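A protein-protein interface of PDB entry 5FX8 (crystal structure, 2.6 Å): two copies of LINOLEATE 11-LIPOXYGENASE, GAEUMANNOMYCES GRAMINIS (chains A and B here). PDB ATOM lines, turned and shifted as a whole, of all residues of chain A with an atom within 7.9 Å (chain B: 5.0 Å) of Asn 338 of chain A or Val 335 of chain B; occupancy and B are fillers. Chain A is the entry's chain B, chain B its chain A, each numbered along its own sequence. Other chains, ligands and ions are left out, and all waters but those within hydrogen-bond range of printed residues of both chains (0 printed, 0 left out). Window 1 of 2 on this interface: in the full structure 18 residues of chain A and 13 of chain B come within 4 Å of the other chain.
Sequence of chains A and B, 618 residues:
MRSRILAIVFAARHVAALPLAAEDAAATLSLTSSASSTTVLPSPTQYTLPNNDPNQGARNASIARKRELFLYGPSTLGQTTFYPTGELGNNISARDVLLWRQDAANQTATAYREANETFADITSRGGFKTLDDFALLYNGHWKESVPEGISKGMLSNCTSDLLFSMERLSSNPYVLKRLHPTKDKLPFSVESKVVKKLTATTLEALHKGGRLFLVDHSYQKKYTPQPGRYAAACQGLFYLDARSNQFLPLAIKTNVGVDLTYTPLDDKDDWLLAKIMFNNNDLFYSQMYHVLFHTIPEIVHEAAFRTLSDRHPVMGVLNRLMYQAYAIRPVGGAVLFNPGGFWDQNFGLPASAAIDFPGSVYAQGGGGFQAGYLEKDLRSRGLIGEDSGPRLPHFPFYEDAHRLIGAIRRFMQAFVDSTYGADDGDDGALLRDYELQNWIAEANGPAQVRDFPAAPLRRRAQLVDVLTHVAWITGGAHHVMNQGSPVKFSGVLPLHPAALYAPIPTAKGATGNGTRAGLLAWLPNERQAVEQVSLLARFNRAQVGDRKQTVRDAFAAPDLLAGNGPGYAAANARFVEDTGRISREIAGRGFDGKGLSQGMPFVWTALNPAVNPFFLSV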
ATOM      1  N   LEU A  77      -8.512  17.541 -25.559  1.00  0.00           N
ATOM      2  CA  LEU A  77      -9.828  17.249 -26.139  1.00  0.00           C
ATOM      3  C   LEU A  77     -10.380  15.922 -25.644  1.00  0.00           C
ATOM      4  O   LEU A  77     -10.833  15.086 -26.419  1.00  0.00           O
ATOM      5  CB  LEU A  77      -9.781  17.256 -27.659  1.00  0.00           C
ATOM      6  CG  LEU A  77     -11.106  17.623 -28.315  1.00  0.00           C
ATOM      7  CD1 LEU A  77     -11.302  19.127 -28.220  1.00  0.00           C
ATOM      8  CD2 LEU A  77     -11.108  17.164 -29.752  1.00  0.00           C
ATOM      9  N   PRO A 330      -6.419  21.627 -30.580  1.00  0.00           N
ATOM     10  CA  PRO A 330      -6.414  23.008 -30.053  1.00  0.00           C
ATOM     11  C   PRO A 330      -7.562  23.857 -30.548  1.00  0.00           C
ATOM     12  O   PRO A 330      -8.207  24.525 -29.752  1.00  0.00           O
ATOM     13  CB  PRO A 330      -5.071  23.551 -30.542  1.00  0.00           C
ATOM     14  CG  PRO A 330      -4.247  22.365 -30.752  1.00  0.00           C
ATOM     15  CD  PRO A 330      -5.155  21.335 -31.276  1.00  0.00           C
ATOM     16  N   VAL A 331      -7.831  23.859 -31.845  1.00  0.00           N
ATOM     17  CA  VAL A 331      -8.939  24.644 -32.371  1.00  0.00           C
ATOM     18  C   VAL A 331     -10.263  24.178 -31.770  1.00  0.00           C
ATOM     19  O   VAL A 331     -11.075  24.997 -31.308  1.00  0.00           O
ATOM     20  CB  VAL A 331      -8.947  24.570 -33.903  1.00  0.00           C
ATOM     21  CG1 VAL A 331     -10.205  25.124 -34.442  1.00  0.00           C
ATOM     22  CG2 VAL A 331      -7.782  25.328 -34.453  1.00  0.00           C
ATOM     23  N   GLY A 332     -10.493  22.855 -31.752  1.00  0.00           N
ATOM     24  CA  GLY A 332     -11.708  22.332 -31.146  1.00  0.00           C
ATOM     25  C   GLY A 332     -11.818  22.696 -29.680  1.00  0.00           C
ATOM     26  O   GLY A 332     -12.902  23.017 -29.183  1.00  0.00           O
ATOM     27  N   GLY A 333     -10.685  22.709 -28.982  1.00  0.00           N
ATOM     28  CA  GLY A 333     -10.692  23.152 -27.603  1.00  0.00           C
ATOM     29  C   GLY A 333     -11.031  24.616 -27.440  1.00  0.00           C
ATOM     30  O   GLY A 333     -11.644  25.003 -26.451  1.00  0.00           O
ATOM     31  N   ALA A 334     -10.628  25.450 -28.390  1.00  0.00           N
ATOM     32  CA  ALA A 334     -10.803  26.883 -28.217  1.00  0.00           C
ATOM     33  C   ALA A 334     -12.161  27.391 -28.684  1.00  0.00           C
ATOM     34  O   ALA A 334     -12.646  28.381 -28.145  1.00  0.00           O
ATOM     35  CB  ALA A 334      -9.702  27.641 -28.953  1.00  0.00           C
ATOM     36  N   VAL A 335     -12.778  26.781 -29.688  1.00  0.00           N
ATOM     37  CA  VAL A 335     -14.012  27.326 -30.226  1.00  0.00           C
ATOM     38  C   VAL A 335     -15.131  26.313 -30.290  1.00  0.00           C
ATOM     39  O   VAL A 335     -16.294  26.717 -30.425  1.00  0.00           O
ATOM     40  CB  VAL A 335     -13.795  27.963 -31.613  1.00  0.00           C
ATOM     41  CG1 VAL A 335     -12.517  28.730 -31.626  1.00  0.00           C
ATOM     42  CG2 VAL A 335     -13.790  26.936 -32.696  1.00  0.00           C
ATOM     43  N   LEU A 336     -14.862  25.018 -30.193  1.00  0.00           N
ATOM     44  CA  LEU A 336     -15.954  24.064 -30.241  1.00  0.00           C
ATOM     45  C   LEU A 336     -16.390  23.625 -28.859  1.00  0.00           C
ATOM     46  O   LEU A 336     -17.570  23.753 -28.515  1.00  0.00           O
ATOM     47  CB  LEU A 336     -15.558  22.852 -31.074  1.00  0.00           C
ATOM     48  CG  LEU A 336     -16.569  21.749 -31.340  1.00  0.00           C
ATOM     49  CD1 LEU A 336     -17.942  22.270 -31.689  1.00  0.00           C
ATOM     50  CD2 LEU A 336     -16.026  20.914 -32.473  1.00  0.00           C
ATOM     51  N   PHE A 337     -15.456  23.132 -28.050  1.00  0.00           N
ATOM     52  CA  PHE A 337     -15.774  22.583 -26.743  1.00  0.00           C
ATOM     53  C   PHE A 337     -15.370  23.497 -25.586  1.00  0.00           C
ATOM     54  O   PHE A 337     -15.484  23.090 -24.425  1.00  0.00           O
ATOM     55  CB  PHE A 337     -15.145  21.195 -26.577  1.00  0.00           C
ATOM     56  CG  PHE A 337     -15.579  20.211 -27.610  1.00  0.00           C
ATOM     57  CD1 PHE A 337     -16.815  19.614 -27.550  1.00  0.00           C
ATOM     58  CD2 PHE A 337     -14.753  19.896 -28.656  1.00  0.00           C
ATOM     59  CE1 PHE A 337     -17.211  18.728 -28.506  1.00  0.00           C
ATOM     60  CE2 PHE A 337     -15.137  19.021 -29.609  1.00  0.00           C
ATOM     61  CZ  PHE A 337     -16.364  18.432 -29.540  1.00  0.00           C
ATOM     62  N   ASN A 338     -14.955  24.726 -25.854  1.00  0.00           N
ATOM     63  CA  ASN A 338     -14.810  25.687 -24.773  1.00  0.00           C
ATOM     64  C   ASN A 338     -16.175  26.029 -24.163  1.00  0.00           C
ATOM     65  O   ASN A 338     -17.195  26.023 -24.857  1.00  0.00           O
ATOM     66  CB  ASN A 338     -14.196  26.954 -25.296  1.00  0.00           C
ATOM     67  CG  ASN A 338     -14.973  27.475 -26.434  1.00  0.00           C
ATOM     68  OD1 ASN A 338     -15.310  26.707 -27.313  1.00  0.00           O
ATOM     69  ND2 ASN A 338     -15.335  28.740 -26.406  1.00  0.00           N
ATOM     70  N   PRO A 339     -16.213  26.389 -22.879  1.00  0.00           N
ATOM     71  CA  PRO A 339     -17.495  26.737 -22.242  1.00  0.00           C
ATOM     72  C   PRO A 339     -18.176  27.894 -22.962  1.00  0.00           C
ATOM     73  O   PRO A 339     -17.605  28.971 -23.135  1.00  0.00           O
ATOM     74  CB  PRO A 339     -17.086  27.129 -20.817  1.00  0.00           C
ATOM     75  CG  PRO A 339     -15.752  26.595 -20.622  1.00  0.00           C
ATOM     76  CD  PRO A 339     -15.083  26.559 -21.954  1.00  0.00           C
ATOM     77  N   GLY A 340     -19.405  27.655 -23.397  1.00  0.00           N
ATOM     78  CA  GLY A 340     -20.112  28.635 -24.187  1.00  0.00           C
ATOM     79  C   GLY A 340     -19.769  28.668 -25.661  1.00  0.00           C
ATOM     80  O   GLY A 340     -20.177  29.616 -26.338  1.00  0.00           O
ATOM     81  N   GLY A 341     -19.036  27.675 -26.179  1.00  0.00           N
ATOM     82  CA  GLY A 341     -18.724  27.603 -27.586  1.00  0.00           C
ATOM     83  C   GLY A 341     -19.839  26.960 -28.397  1.00  0.00           C
ATOM     84  O   GLY A 341     -20.964  26.754 -27.934  1.00  0.00           O
ATOM     85  N   PHE A 342     -19.491  26.609 -29.638  1.00  0.00           N
ATOM     86  CA  PHE A 342     -20.512  26.180 -30.591  1.00  0.00           C
ATOM     87  C   PHE A 342     -21.174  24.864 -30.202  1.00  0.00           C
ATOM     88  O   PHE A 342     -22.320  24.627 -30.581  1.00  0.00           O
ATOM     89  CB  PHE A 342     -19.919  26.074 -31.990  1.00  0.00           C
ATOM     90  CG  PHE A 342     -19.539  27.380 -32.571  1.00  0.00           C
ATOM     91  CD1 PHE A 342     -20.504  28.305 -32.898  1.00  0.00           C
ATOM     92  CD2 PHE A 342     -18.218  27.691 -32.789  1.00  0.00           C
ATOM     93  CE1 PHE A 342     -20.152  29.518 -33.422  1.00  0.00           C
ATOM     94  CE2 PHE A 342     -17.858  28.908 -33.312  1.00  0.00           C
ATOM     95  CZ  PHE A 342     -18.818  29.820 -33.636  1.00  0.00           C
ATOM     96  N   TRP A 343     -20.491  23.995 -29.468  1.00  0.00           N
ATOM     97  CA  TRP A 343     -21.171  22.796 -29.010  1.00  0.00           C
ATOM     98  C   TRP A 343     -22.217  23.149 -27.954  1.00  0.00           C
ATOM     99  O   TRP A 343     -23.390  22.790 -28.091  1.00  0.00           O
ATOM    100  CB  TRP A 343     -20.162  21.760 -28.496  1.00  0.00           C
ATOM    101  CG  TRP A 343     -20.840  20.556 -27.932  1.00  0.00           C
ATOM    102  CD1 TRP A 343     -21.368  20.432 -26.684  1.00  0.00           C
ATOM    103  CD2 TRP A 343     -21.090  19.311 -28.590  1.00  0.00           C
ATOM    104  NE1 TRP A 343     -21.946  19.207 -26.528  1.00  0.00           N
ATOM    105  CE2 TRP A 343     -21.774  18.490 -27.680  1.00  0.00           C
ATOM    106  CE3 TRP A 343     -20.799  18.811 -29.849  1.00  0.00           C
ATOM    107  CZ2 TRP A 343     -22.171  17.195 -27.995  1.00  0.00           C
ATOM    108  CZ3 TRP A 343     -21.208  17.540 -30.162  1.00  0.00           C
ATOM    109  CH2 TRP A 343     -21.881  16.740 -29.241  1.00  0.00           C
ATOM    110  N   ASP A 344     -21.818  23.889 -26.911  1.00  0.00           N
ATOM    111  CA  ASP A 344     -22.782  24.382 -25.933  1.00  0.00           C
ATOM    112  C   ASP A 344     -23.946  25.100 -26.606  1.00  0.00           C
ATOM    113  O   ASP A 344     -25.104  24.882 -26.257  1.00  0.00           O
ATOM    114  CB  ASP A 344     -22.101  25.315 -24.939  1.00  0.00           C
ATOM    115  CG  ASP A 344     -21.236  24.581 -23.942  1.00  0.00           C
ATOM    116  OD1 ASP A 344     -21.453  23.374 -23.740  1.00  0.00           O
ATOM    117  OD2 ASP A 344     -20.354  25.225 -23.351  1.00  0.00           O
ATOM    118  N   GLN A 345     -23.664  25.926 -27.603  1.00  0.00           N
ATOM    119  CA  GLN A 345     -24.729  26.693 -28.222  1.00  0.00           C
ATOM    120  C   GLN A 345     -25.743  25.835 -28.965  1.00  0.00           C
ATOM    121  O   GLN A 345     -26.840  26.318 -29.236  1.00  0.00           O
ATOM    122  CB  GLN A 345     -24.137  27.710 -29.171  1.00  0.00           C
ATOM    123  CG  GLN A 345     -25.050  28.848 -29.451  1.00  0.00           C
ATOM    124  CD  GLN A 345     -24.667  29.607 -30.692  1.00  0.00           C
ATOM    125  OE1 GLN A 345     -23.774  29.200 -31.444  1.00  0.00           O
ATOM    126  NE2 GLN A 345     -25.332  30.739 -30.910  1.00  0.00           N
ATOM    127  N   ALA A 351     -20.685  20.635 -23.272  1.00  0.00           N
ATOM    128  CA  ALA A 351     -19.399  20.217 -23.836  1.00  0.00           C
ATOM    129  C   ALA A 351     -18.587  19.399 -22.852  1.00  0.00           C
ATOM    130  O   ALA A 351     -17.690  18.655 -23.260  1.00  0.00           O
ATOM    131  CB  ALA A 351     -18.565  21.415 -24.301  1.00  0.00           C
ATOM    132  N   SER A 352     -18.892  19.506 -21.570  1.00  0.00           N
ATOM    133  CA  SER A 352     -18.167  18.712 -20.598  1.00  0.00           C
ATOM    134  C   SER A 352     -18.500  17.226 -20.746  1.00  0.00           C
ATOM    135  O   SER A 352     -17.607  16.376 -20.661  1.00  0.00           O
ATOM    136  CB  SER A 352     -18.495  19.239 -19.208  1.00  0.00           C
ATOM    137  OG  SER A 352     -19.898  19.345 -19.084  1.00  0.00           O
ATOM    138  N   ILE A 355     -16.973  16.006 -24.145  1.00  0.00           N
ATOM    139  CA  ILE A 355     -15.550  15.728 -23.993  1.00  0.00           C
ATOM    140  C   ILE A 355     -15.321  14.468 -23.180  1.00  0.00           C
ATOM    141  O   ILE A 355     -14.365  13.725 -23.425  1.00  0.00           O
ATOM    142  CB  ILE A 355     -14.856  16.949 -23.363  1.00  0.00           C
ATOM    143  CG1 ILE A 355     -14.652  18.027 -24.426  1.00  0.00           C
ATOM    144  CG2 ILE A 355     -13.557  16.580 -22.687  1.00  0.00           C
ATOM    145  CD1 ILE A 355     -14.046  17.512 -25.732  1.00  0.00           C
ATOM    146  N   THR B 108     -20.653  34.875 -27.460  1.00  0.00           N
ATOM    147  CA  THR B 108     -19.519  34.307 -28.183  1.00  0.00           C
ATOM    148  C   THR B 108     -19.834  34.132 -29.659  1.00  0.00           C
ATOM    149  O   THR B 108     -19.057  34.553 -30.530  1.00  0.00           O
ATOM    150  CB  THR B 108     -19.124  32.970 -27.588  1.00  0.00           C
ATOM    151  OG1 THR B 108     -18.973  33.099 -26.186  1.00  0.00           O
ATOM    152  CG2 THR B 108     -17.817  32.553 -28.146  1.00  0.00           C
ATOM    153  N   VAL B 331     -12.979  28.414 -15.772  1.00  0.00           N
ATOM    154  CA  VAL B 331     -13.128  28.726 -17.185  1.00  0.00           C
ATOM    155  C   VAL B 331     -11.870  29.405 -17.692  1.00  0.00           C
ATOM    156  O   VAL B 331     -11.334  29.055 -18.753  1.00  0.00           O
ATOM    157  CB  VAL B 331     -14.384  29.589 -17.412  1.00  0.00           C
ATOM    158  CG1 VAL B 331     -14.431  30.150 -18.820  1.00  0.00           C
ATOM    159  CG2 VAL B 331     -15.631  28.783 -17.136  1.00  0.00           C
ATOM    160  N   GLY B 332     -11.354  30.351 -16.913  1.00  0.00           N
ATOM    161  CA  GLY B 332     -10.130  31.026 -17.294  1.00  0.00           C
ATOM    162  C   GLY B 332      -8.954  30.079 -17.401  1.00  0.00           C
ATOM    163  O   GLY B 332      -8.153  30.172 -18.326  1.00  0.00           O
ATOM    164  N   GLY B 333      -8.849  29.135 -16.473  1.00  0.00           N
ATOM    165  CA  GLY B 333      -7.792  28.154 -16.564  1.00  0.00           C
ATOM    166  C   GLY B 333      -7.929  27.218 -17.743  1.00  0.00           C
ATOM    167  O   GLY B 333      -6.927  26.713 -18.251  1.00  0.00           O
ATOM    168  N   ALA B 334      -9.155  26.962 -18.191  1.00  0.00           N
ATOM    169  CA  ALA B 334      -9.328  25.979 -19.248  1.00  0.00           C
ATOM    170  C   ALA B 334      -9.235  26.577 -20.643  1.00  0.00           C
ATOM    171  O   ALA B 334      -8.842  25.879 -21.576  1.00  0.00           O
ATOM    172  CB  ALA B 334     -10.672  25.261 -19.082  1.00  0.00           C
ATOM    173  N   VAL B 335      -9.587  27.845 -20.835  1.00  0.00           N
ATOM    174  CA  VAL B 335      -9.553  28.396 -22.185  1.00  0.00           C
ATOM    175  C   VAL B 335      -8.779  29.684 -22.285  1.00  0.00           C
ATOM    176  O   VAL B 335      -8.403  30.083 -23.396  1.00  0.00           O
ATOM    177  CB  VAL B 335     -10.976  28.596 -22.758  1.00  0.00           C
ATOM    178  CG1 VAL B 335     -11.725  27.296 -22.797  1.00  0.00           C
ATOM    179  CG2 VAL B 335     -11.727  29.583 -21.964  1.00  0.00           C
ATOM    180  N   LEU B 336      -8.490  30.378 -21.204  1.00  0.00           N
ATOM    181  CA  LEU B 336      -7.852  31.674 -21.342  1.00  0.00           C
ATOM    182  C   LEU B 336      -6.350  31.602 -21.117  1.00  0.00           C
ATOM    183  O   LEU B 336      -5.571  32.030 -21.968  1.00  0.00           O
ATOM    184  CB  LEU B 336      -8.495  32.665 -20.366  1.00  0.00           C
ATOM    185  CG  LEU B 336      -8.043  34.114 -20.422  1.00  0.00           C
ATOM    186  CD1 LEU B 336      -8.081  34.577 -21.846  1.00  0.00           C
ATOM    187  CD2 LEU B 336      -8.958  34.932 -19.555  1.00  0.00           C
ATOM    188  N   PHE B 337      -5.927  31.034 -19.994  1.00  0.00           N
ATOM    189  CA  PHE B 337      -4.521  31.029 -19.621  1.00  0.00           C
ATOM    190  C   PHE B 337      -3.874  29.665 -19.790  1.00  0.00           C
ATOM    191  O   PHE B 337      -2.779  29.446 -19.274  1.00  0.00           O
ATOM    192  CB  PHE B 337      -4.346  31.538 -18.189  1.00  0.00           C
ATOM    193  CG  PHE B 337      -4.849  32.916 -17.989  1.00  0.00           C
ATOM    194  CD1 PHE B 337      -4.195  33.990 -18.547  1.00  0.00           C
ATOM    195  CD2 PHE B 337      -5.999  33.148 -17.256  1.00  0.00           C
ATOM    196  CE1 PHE B 337      -4.673  35.267 -18.365  1.00  0.00           C
ATOM    197  CE2 PHE B 337      -6.476  34.423 -17.071  1.00  0.00           C
ATOM    198  CZ  PHE B 337      -5.817  35.475 -17.627  1.00  0.00           C
ATOM    199  N   ASN B 338      -4.524  28.747 -20.507  1.00  0.00           N
ATOM    200  CA  ASN B 338      -3.928  27.480 -20.876  1.00  0.00           C
ATOM    201  C   ASN B 338      -2.914  27.666 -22.000  1.00  0.00           C
ATOM    202  O   ASN B 338      -2.951  28.656 -22.733  1.00  0.00           O
ATOM    203  CB  ASN B 338      -5.008  26.503 -21.311  1.00  0.00           C
ATOM    204  CG  ASN B 338      -5.800  27.013 -22.483  1.00  0.00           C
ATOM    205  OD1 ASN B 338      -6.486  28.013 -22.367  1.00  0.00           O
ATOM    206  ND2 ASN B 338      -5.708  26.335 -23.619  1.00  0.00           N
ATOM    207  N   GLY B 341      -4.112  29.177 -25.326  1.00  0.00           N
ATOM    208  CA  GLY B 341      -5.434  29.717 -25.188  1.00  0.00           C
ATOM    209  C   GLY B 341      -5.484  31.139 -25.688  1.00  0.00           C
ATOM    210  O   GLY B 341      -4.559  31.652 -26.315  1.00  0.00           O
ATOM    211  N   PHE B 342      -6.588  31.797 -25.353  1.00  0.00           N
ATOM    212  CA  PHE B 342      -6.883  33.093 -25.939  1.00  0.00           C
ATOM    213  C   PHE B 342      -5.868  34.140 -25.536  1.00  0.00           C
ATOM    214  O   PHE B 342      -5.558  35.056 -26.320  1.00  0.00           O
ATOM    215  CB  PHE B 342      -8.265  33.529 -25.523  1.00  0.00           C
ATOM    216  CG  PHE B 342      -9.327  32.631 -25.990  1.00  0.00           C
ATOM    217  CD1 PHE B 342      -9.476  32.361 -27.324  1.00  0.00           C
ATOM    218  CD2 PHE B 342     -10.208  32.073 -25.098  1.00  0.00           C
ATOM    219  CE1 PHE B 342     -10.473  31.558 -27.757  1.00  0.00           C
ATOM    220  CE2 PHE B 342     -11.215  31.260 -25.542  1.00  0.00           C
ATOM    221  CZ  PHE B 342     -11.327  30.999 -26.882  1.00  0.00           C
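The side-chain amide oxygen (OD1) of Asn 338 of chain B sits close to the backbone carbonyl oxygen (O) of Val 335 of chain B (3.0 Å). The backbone carbonyl oxygen of Gly 333 of chain A lies within hydrogen-bond range of the backbone NH of Asn 338 of chain A (3.4 Å). ND2 of Asn 338 of chain A sits close to O of Ala 334 of chain A (3.2 Å). OD1 of Asn 338 of chain A lies close to O of Val 335 of chain A (3.3 Å). OD1 of Asn 338 of chain A is in hydrogen-bond range of N of Leu 336 of chain A (3.4 Å). The backbone NH (N) of Gly 340 of chain A is in hydrogen-bond range of the side-chain carboxylate (OD2) of Asp 344 of chain A (2.6 Å).
Printed residues of chain A that touch a printed residue of chain B: Ala 334, Asn 338, Pro 339 and Gly 340. Hydrophobic or aromatic side chains of chain A within 4 Å of the printed part of chain B: Pro 339. Of the 11 printed residues of chain B, 3 touch a printed residue of chain A. Along chain B the printed residues that touch a printed residue of chain A span positions 108 to 342. Among the printed residues, 4 pairs touch across the chains. Among the printed residues, no Asp or Glu carboxylate lies within 4 Å of a Lys or Arg side-chain nitrogen of the other chain.
Ala 334 of chain A touches Phe 342 of chain B. Val 335 of chain B touches Asn 338 of chain A (CG1 to CB, 3.5 Å). Pro 339 of chain A touches Val 335 of chain B (CD to CG1, 3.5 Å). O of Gly 340 of chain A touches OG1 of Thr 108 of chain B, 3.7 Å away.
Leu 77 of chain A touches none of the printed residues of chain B. Printed residues of chain B within 4 Å of Ala 334 of chain A: Phe 342. Asn 338 of chain A touches one residue of chain B. Of the printed residues of chain B, Pro 339 of chain A touches Val 335 (3.5 Å). Printed residues of chain A within 4 Å of Thr 108 of chain B: Gly 340 (3.7 Å). No residue of chain A comes within 4 Å of Ala 334 of chain B. Of the printed residues of chain A, Phe 342 of chain B touches Ala 334. The nearest residue of chain A that does not touch Val 335 of chain B is Gly 333 of chain A (4.3 Å).
Ala 334 of chain A touches Phe 342 of chain B, but with the chains exchanged Phe 342 of chain A does not touch Ala 334 of chain B (13.4 Å). Asn 338 of chain A touches Val 335 of chain B, but with the chains exchanged Val 335 of chain A does not touch Asn 338 of chain B (9.3 Å). Of the 4 pairs that touch across the chains among the printed residues, none has its exchanged pair printed and touching as well.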
